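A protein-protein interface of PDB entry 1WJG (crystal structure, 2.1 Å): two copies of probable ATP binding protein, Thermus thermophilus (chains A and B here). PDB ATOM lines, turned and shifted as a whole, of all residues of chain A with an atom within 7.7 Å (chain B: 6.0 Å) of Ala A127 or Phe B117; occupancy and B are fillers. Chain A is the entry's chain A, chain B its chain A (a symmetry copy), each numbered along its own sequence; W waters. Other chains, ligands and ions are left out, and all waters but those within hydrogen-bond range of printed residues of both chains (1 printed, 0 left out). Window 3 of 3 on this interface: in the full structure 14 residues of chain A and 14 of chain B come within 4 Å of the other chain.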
ATOM      1  N   LEU A  92      16.582   7.365 -28.753  1.00  0.00           N
ATOM      2  CA  LEU A  92      17.153   8.263 -27.742  1.00  0.00           C
ATOM      3  C   LEU A  92      16.086   9.188 -27.168  1.00  0.00           C
ATOM      4  O   LEU A  92      16.074   9.475 -25.974  1.00  0.00           O
ATOM      5  CB  LEU A  92      18.294   9.108 -28.329  1.00  0.00           C
ATOM      6  CG  LEU A  92      19.745   8.604 -28.318  1.00  0.00           C
ATOM      7  CD1 LEU A  92      19.904   7.412 -27.400  1.00  0.00           C
ATOM      8  CD2 LEU A  92      20.199   8.264 -29.721  1.00  0.00           C
ATOM      9  N   PHE A 117      29.082  -5.049 -38.991  1.00  0.00           N
ATOM     10  CA  PHE A 117      29.522  -4.894 -37.601  1.00  0.00           C
ATOM     11  C   PHE A 117      28.407  -4.323 -36.725  1.00  0.00           C
ATOM     12  O   PHE A 117      28.018  -4.925 -35.725  1.00  0.00           O
ATOM     13  CB  PHE A 117      30.756  -3.978 -37.537  1.00  0.00           C
ATOM     14  CG  PHE A 117      31.079  -3.482 -36.151  1.00  0.00           C
ATOM     15  CD1 PHE A 117      31.275  -4.376 -35.104  1.00  0.00           C
ATOM     16  CD2 PHE A 117      31.142  -2.118 -35.889  1.00  0.00           C
ATOM     17  CE1 PHE A 117      31.524  -3.917 -33.814  1.00  0.00           C
ATOM     18  CE2 PHE A 117      31.391  -1.651 -34.602  1.00  0.00           C
ATOM     19  CZ  PHE A 117      31.581  -2.550 -33.564  1.00  0.00           C
ATOM     20  N   LEU A 118      27.903  -3.158 -37.114  1.00  0.00           N
ATOM     21  CA  LEU A 118      26.854  -2.479 -36.372  1.00  0.00           C
ATOM     22  C   LEU A 118      25.983  -1.674 -37.307  1.00  0.00           C
ATOM     23  O   LEU A 118      26.480  -1.052 -38.251  1.00  0.00           O
ATOM     24  CB  LEU A 118      27.454  -1.487 -35.367  1.00  0.00           C
ATOM     25  CG  LEU A 118      27.738  -1.842 -33.909  1.00  0.00           C
ATOM     26  CD1 LEU A 118      28.406  -0.648 -33.240  1.00  0.00           C
ATOM     27  CD2 LEU A 118      26.449  -2.173 -33.192  1.00  0.00           C
ATOM     28  N   GLY A 119      24.687  -1.664 -37.010  1.00  0.00           N
ATOM     29  CA  GLY A 119      23.754  -0.881 -37.791  1.00  0.00           C
ATOM     30  C   GLY A 119      24.005   0.574 -37.440  1.00  0.00           C
ATOM     31  O   GLY A 119      24.535   0.882 -36.365  1.00  0.00           O
ATOM     32  N   SER A 120      23.663   1.479 -38.348  1.00  0.00           N
ATOM     33  CA  SER A 120      23.875   2.901 -38.094  1.00  0.00           C
ATOM     34  C   SER A 120      23.120   3.355 -36.840  1.00  0.00           C
ATOM     35  O   SER A 120      23.629   4.145 -36.048  1.00  0.00           O
ATOM     36  CB  SER A 120      23.441   3.734 -39.308  1.00  0.00           C
ATOM     37  OG  SER A 120      22.090   3.469 -39.650  1.00  0.00           O
ATOM     38  N   GLN A 121      21.936   2.788 -36.635  1.00  0.00           N
ATOM     39  CA  GLN A 121      21.105   3.136 -35.492  1.00  0.00           C
ATOM     40  C   GLN A 121      21.662   2.635 -34.172  1.00  0.00           C
ATOM     41  O   GLN A 121      21.722   3.383 -33.200  1.00  0.00           O
ATOM     42  CB  GLN A 121      19.672   2.669 -35.722  1.00  0.00           C
ATOM     43  CG  GLN A 121      19.092   3.206 -37.038  1.00  0.00           C
ATOM     44  CD  GLN A 121      19.384   4.699 -37.260  1.00  0.00           C
ATOM     45  OE1 GLN A 121      18.699   5.570 -36.728  1.00  0.00           O
ATOM     46  NE2 GLN A 121      20.401   4.988 -38.065  1.00  0.00           N
ATOM     47  N   SER A 122      22.093   1.379 -34.140  1.00  0.00           N
ATOM     48  CA  SER A 122      22.675   0.829 -32.923  1.00  0.00           C
ATOM     49  C   SER A 122      23.969   1.593 -32.607  1.00  0.00           C
ATOM     50  O   SER A 122      24.297   1.808 -31.443  1.00  0.00           O
ATOM     51  CB  SER A 122      22.946  -0.664 -33.090  1.00  0.00           C
ATOM     52  OG  SER A 122      23.754  -0.898 -34.232  1.00  0.00           O
ATOM     53  N   GLN A 123      24.675   2.040 -33.645  1.00  0.00           N
ATOM     54  CA  GLN A 123      25.909   2.795 -33.439  1.00  0.00           C
ATOM     55  C   GLN A 123      25.622   4.143 -32.780  1.00  0.00           C
ATOM     56  O   GLN A 123      26.340   4.552 -31.873  1.00  0.00           O
ATOM     57  CB  GLN A 123      26.675   3.006 -34.748  1.00  0.00           C
ATOM     58  CG  GLN A 123      27.952   3.841 -34.563  1.00  0.00           C
ATOM     59  CD  GLN A 123      28.883   3.817 -35.765  1.00  0.00           C
ATOM     60  OE1 GLN A 123      28.786   2.943 -36.630  1.00  0.00           O
ATOM     61  NE2 GLN A 123      29.807   4.772 -35.814  1.00  0.00           N
ATOM     62  N   ARG A 124      24.563   4.820 -33.220  1.00  0.00           N
ATOM     63  CA  ARG A 124      24.215   6.112 -32.639  1.00  0.00           C
ATOM     64  C   ARG A 124      23.732   5.946 -31.195  1.00  0.00           C
ATOM     65  O   ARG A 124      24.040   6.770 -30.338  1.00  0.00           O
ATOM     66  CB  ARG A 124      23.157   6.826 -33.487  1.00  0.00           C
ATOM     67  CG  ARG A 124      22.568   8.071 -32.833  1.00  0.00           C
ATOM     68  CD  ARG A 124      23.059   9.386 -33.431  1.00  0.00           C
ATOM     69  NE  ARG A 124      22.406  10.518 -32.769  1.00  0.00           N
ATOM     70  CZ  ARG A 124      21.243  11.054 -33.139  1.00  0.00           C
ATOM     71  NH1 ARG A 124      20.733  12.067 -32.452  1.00  0.00           N
ATOM     72  NH2 ARG A 124      20.607  10.613 -34.219  1.00  0.00           N
ATOM     73  N   VAL A 125      23.005   4.863 -30.925  1.00  0.00           N
ATOM     74  CA  VAL A 125      22.506   4.601 -29.577  1.00  0.00           C
ATOM     75  C   VAL A 125      23.661   4.269 -28.629  1.00  0.00           C
ATOM     76  O   VAL A 125      23.717   4.784 -27.516  1.00  0.00           O
ATOM     77  CB  VAL A 125      21.462   3.455 -29.563  1.00  0.00           C
ATOM     78  CG1 VAL A 125      21.063   3.108 -28.138  1.00  0.00           C
ATOM     79  CG2 VAL A 125      20.237   3.860 -30.356  1.00  0.00           C
ATOM     80  N   VAL A 126      24.578   3.416 -29.076  1.00  0.00           N
ATOM     81  CA  VAL A 126      25.737   3.046 -28.260  1.00  0.00           C
ATOM     82  C   VAL A 126      26.605   4.276 -28.003  1.00  0.00           C
ATOM     83  O   VAL A 126      27.202   4.420 -26.930  1.00  0.00           O
ATOM     84  CB  VAL A 126      26.575   1.930 -28.940  1.00  0.00           C
ATOM     85  CG1 VAL A 126      27.873   1.679 -28.159  1.00  0.00           C
ATOM     86  CG2 VAL A 126      25.762   0.644 -28.997  1.00  0.00           C
ATOM     87  N   ALA A 127      26.625   5.187 -28.972  1.00  0.00           N
ATOM     88  CA  ALA A 127      27.406   6.410 -28.857  1.00  0.00           C
ATOM     89  C   ALA A 127      26.804   7.488 -27.955  1.00  0.00           C
ATOM     90  O   ALA A 127      27.542   8.157 -27.230  1.00  0.00           O
ATOM     91  CB  ALA A 127      27.679   6.996 -30.250  1.00  0.00           C
ATOM     92  N   GLU A 128      25.479   7.626 -27.954  1.00  0.00           N
ATOM     93  CA  GLU A 128      24.823   8.685 -27.181  1.00  0.00           C
ATOM     94  C   GLU A 128      23.860   8.336 -26.035  1.00  0.00           C
ATOM     95  O   GLU A 128      23.426   9.237 -25.307  1.00  0.00           O
ATOM     96  CB  GLU A 128      24.113   9.644 -28.147  1.00  0.00           C
ATOM     97  CG  GLU A 128      25.021  10.228 -29.229  1.00  0.00           C
ATOM     98  CD  GLU A 128      24.276  11.067 -30.261  1.00  0.00           C
ATOM     99  OE1 GLU A 128      24.901  11.435 -31.281  1.00  0.00           O
ATOM    100  OE2 GLU A 128      23.075  11.364 -30.067  1.00  0.00           O
ATOM    101  N   ALA A 129      23.504   7.064 -25.872  1.00  0.00           N
ATOM    102  CA  ALA A 129      22.584   6.687 -24.797  1.00  0.00           C
ATOM    103  C   ALA A 129      23.250   6.722 -23.427  1.00  0.00           C
ATOM    104  O   ALA A 129      24.350   6.207 -23.253  1.00  0.00           O
ATOM    105  CB  ALA A 129      21.998   5.303 -25.052  1.00  0.00           C
ATOM    106  N   PRO A 130      22.591   7.346 -22.437  1.00  0.00           N
ATOM    107  CA  PRO A 130      23.095   7.459 -21.063  1.00  0.00           C
ATOM    108  C   PRO A 130      23.128   6.091 -20.371  1.00  0.00           C
ATOM    109  O   PRO A 130      24.125   5.714 -19.750  1.00  0.00           O
ATOM    110  CB  PRO A 130      22.058   8.366 -20.396  1.00  0.00           C
ATOM    111  CG  PRO A 130      21.511   9.170 -21.528  1.00  0.00           C
ATOM    112  CD  PRO A 130      21.356   8.132 -22.598  1.00  0.00           C
ATOM    113  N   VAL A 133      23.203  -0.495 -22.897  1.00  0.00           N
ATOM    114  CA  VAL A 133      22.584  -0.965 -24.138  1.00  0.00           C
ATOM    115  C   VAL A 133      22.842  -2.455 -24.303  1.00  0.00           C
ATOM    116  O   VAL A 133      23.990  -2.906 -24.275  1.00  0.00           O
ATOM    117  CB  VAL A 133      23.143  -0.220 -25.371  1.00  0.00           C
ATOM    118  CG1 VAL A 133      22.478  -0.732 -26.655  1.00  0.00           C
ATOM    119  CG2 VAL A 133      22.911   1.281 -25.223  1.00  0.00           C
ATOM    120  N   THR B 107      31.510   0.021 -22.219  1.00  0.00           N
ATOM    121  CA  THR B 107      31.532   0.458 -23.617  1.00  0.00           C
ATOM    122  C   THR B 107      32.970   0.826 -23.974  1.00  0.00           C
ATOM    123  O   THR B 107      33.455   0.528 -25.069  1.00  0.00           O
ATOM    124  CB  THR B 107      30.639   1.695 -23.822  1.00  0.00           C
ATOM    125  OG1 THR B 107      29.311   1.398 -23.380  1.00  0.00           O
ATOM    126  CG2 THR B 107      30.602   2.094 -25.300  1.00  0.00           C
ATOM    127  N   ARG B 108      33.649   1.437 -23.007  1.00  0.00           N
ATOM    128  CA  ARG B 108      35.039   1.854 -23.152  1.00  0.00           C
ATOM    129  C   ARG B 108      35.917   1.150 -22.118  1.00  0.00           C
ATOM    130  O   ARG B 108      35.416   0.459 -21.229  1.00  0.00           O
ATOM    131  CB  ARG B 108      35.144   3.368 -22.992  1.00  0.00           C
ATOM    132  CG  ARG B 108      34.375   4.132 -24.065  1.00  0.00           C
ATOM    133  CD  ARG B 108      34.748   5.594 -24.088  1.00  0.00           C
ATOM    134  NE  ARG B 108      34.177   6.335 -22.968  1.00  0.00           N
ATOM    135  CZ  ARG B 108      34.615   7.523 -22.561  1.00  0.00           C
ATOM    136  NH1 ARG B 108      34.032   8.129 -21.535  1.00  0.00           N
ATOM    137  NH2 ARG B 108      35.652   8.093 -23.162  1.00  0.00           N
ATOM    138  N   SER B 115      38.411   4.343 -28.869  1.00  0.00           N
ATOM    139  CA  SER B 115      37.952   5.685 -29.161  1.00  0.00           C
ATOM    140  C   SER B 115      36.972   6.074 -28.062  1.00  0.00           C
ATOM    141  O   SER B 115      36.666   5.267 -27.184  1.00  0.00           O
ATOM    142  CB  SER B 115      37.236   5.711 -30.511  1.00  0.00           C
ATOM    143  OG  SER B 115      36.058   4.927 -30.469  1.00  0.00           O
ATOM    144  N   LEU B 116      36.494   7.311 -28.109  1.00  0.00           N
ATOM    145  CA  LEU B 116      35.511   7.790 -27.145  1.00  0.00           C
ATOM    146  C   LEU B 116      34.171   7.085 -27.408  1.00  0.00           C
ATOM    147  O   LEU B 116      33.263   7.123 -26.576  1.00  0.00           O
ATOM    148  CB  LEU B 116      35.342   9.304 -27.277  1.00  0.00           C
ATOM    149  CG  LEU B 116      36.003  10.229 -26.245  1.00  0.00           C
ATOM    150  CD1 LEU B 116      37.233   9.605 -25.634  1.00  0.00           C
ATOM    151  CD2 LEU B 116      36.309  11.573 -26.885  1.00  0.00           C
ATOM    152  N   PHE B 117      34.061   6.450 -28.574  1.00  0.00           N
ATOM    153  CA  PHE B 117      32.849   5.723 -28.965  1.00  0.00           C
ATOM    154  C   PHE B 117      32.831   4.313 -28.372  1.00  0.00           C
ATOM    155  O   PHE B 117      31.899   3.938 -27.662  1.00  0.00           O
ATOM    156  CB  PHE B 117      32.750   5.647 -30.497  1.00  0.00           C
ATOM    157  CG  PHE B 117      31.742   4.643 -30.996  1.00  0.00           C
ATOM    158  CD1 PHE B 117      30.416   4.701 -30.580  1.00  0.00           C
ATOM    159  CD2 PHE B 117      32.133   3.615 -31.847  1.00  0.00           C
ATOM    160  CE1 PHE B 117      29.495   3.746 -31.001  1.00  0.00           C
ATOM    161  CE2 PHE B 117      31.219   2.657 -32.273  1.00  0.00           C
ATOM    162  CZ  PHE B 117      29.901   2.721 -31.849  1.00  0.00           C
ATOM    163  N   LEU B 118      33.870   3.544 -28.676  1.00  0.00           N
ATOM    164  CA  LEU B 118      33.984   2.173 -28.207  1.00  0.00           C
ATOM    165  C   LEU B 118      35.436   1.798 -28.023  1.00  0.00           C
ATOM    166  O   LEU B 118      36.290   2.176 -28.830  1.00  0.00           O
ATOM    167  CB  LEU B 118      33.404   1.196 -29.238  1.00  0.00           C
ATOM    168  CG  LEU B 118      31.963   0.694 -29.197  1.00  0.00           C
ATOM    169  CD1 LEU B 118      31.720  -0.185 -30.417  1.00  0.00           C
ATOM    170  CD2 LEU B 118      31.724  -0.105 -27.937  1.00  0.00           C
ATOM    171  N   GLY B 119      35.693   1.020 -26.977  1.00  0.00           N
ATOM    172  CA  GLY B 119      37.035   0.539 -26.725  1.00  0.00           C
ATOM    173  C   GLY B 119      37.325  -0.515 -27.776  1.00  0.00           C
ATOM    174  O   GLY B 119      36.402  -1.115 -28.342  1.00  0.00           O
ATOM    175  N   GLN B 123      34.695  -3.431 -29.034  1.00  0.00           N
ATOM    176  CA  GLN B 123      34.408  -3.486 -30.466  1.00  0.00           C
ATOM    177  C   GLN B 123      34.606  -4.900 -31.010  1.00  0.00           C
ATOM    178  O   GLN B 123      33.794  -5.379 -31.794  1.00  0.00           O
ATOM    179  CB  GLN B 123      35.265  -2.495 -31.259  1.00  0.00           C
ATOM    180  CG  GLN B 123      35.015  -2.571 -32.774  1.00  0.00           C
ATOM    181  CD  GLN B 123      35.616  -1.413 -33.555  1.00  0.00           C
ATOM    182  OE1 GLN B 123      35.947  -0.367 -32.993  1.00  0.00           O
ATOM    183  NE2 GLN B 123      35.742  -1.591 -34.867  1.00  0.00           N
HETATM  184  O   HOH W   1      27.266   3.277 -24.367  1.00  0.00           O
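Of the printed residues of chain B, Gln A123 touches Phe B117.
Arg A124 touches none of the printed residues of chain B.
Of the printed residues of chain B, Ala A127 touches Phe B117 (3.6 Å).
Printed residues of chain A within 4 Å of Thr B107: Val A126.
Of chain A, only Leu A118 (3.9 Å), Gln A123 (3.4 Å), Val A126 (3.9 Å) and Ala A127 (3.6 Å) come within 4 Å of Phe B117.
The nearest residue of chain B that does not touch Ala A127 is Leu B116 (5.9 Å).
The nearest printed residue of chain A that does not touch Leu B118 is Val A126 (4.2 Å).
Phe A117 touches Leu B118, and with the chains exchanged Leu A118 touches Phe B117.
Phe A117 touches Gln B123, and with the chains exchanged Gln A123 touches Phe B117.
Of the 7 pairs that touch across the chains among the printed residues, 4 have their exchanged pair printed and touching as well.
CD1 of Leu B118 touches CZ of Phe A117 (3.9 Å).
Gln B123 touches Phe A117 (O to CE1, 3.4 Å).
Leu A118 touches Phe B117 (CD1 to CZ, 3.9 Å).
Gln A123 touches Phe B117.
CG2 of Thr B107 touches CG1 of Val A126, 3.97 Å away.
Val A126 touches Phe B117.
Ala A127 touches Phe B117.
Of the 8 printed residues of chain B, 4 touch a printed residue of chain A.
Of the 16 printed residues of chain A, 5 touch a printed residue of chain B.
Hydrophobic or aromatic side chains of chain A that line the printed part of chain B: Phe A117, Leu A118, Val A126 and Ala A127.
Among the printed residues, 7 pairs touch across the chains.
Among the printed residues, no Asp or Glu carboxylate lies within 4 Å of a Lys or Arg side-chain nitrogen of the other chain.
Water W1 lies within hydrogen-bond range of the backbone carbonyl oxygen (O) of Val A126 and the side-chain hydroxyl (OG1) of Thr B107.
O of Thr B107 sits at hydrogen-bond distance from N of Gly B119 (3.0 Å).
The backbone NH (N) of Phe B117 lies close to the side-chain hydroxyl (OG) of Ser B115, at 3.1 Å.
The side-chain hydroxyl of Ser B115 lies within hydrogen-bond range of the backbone NH of Leu B118 (3.1 Å).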
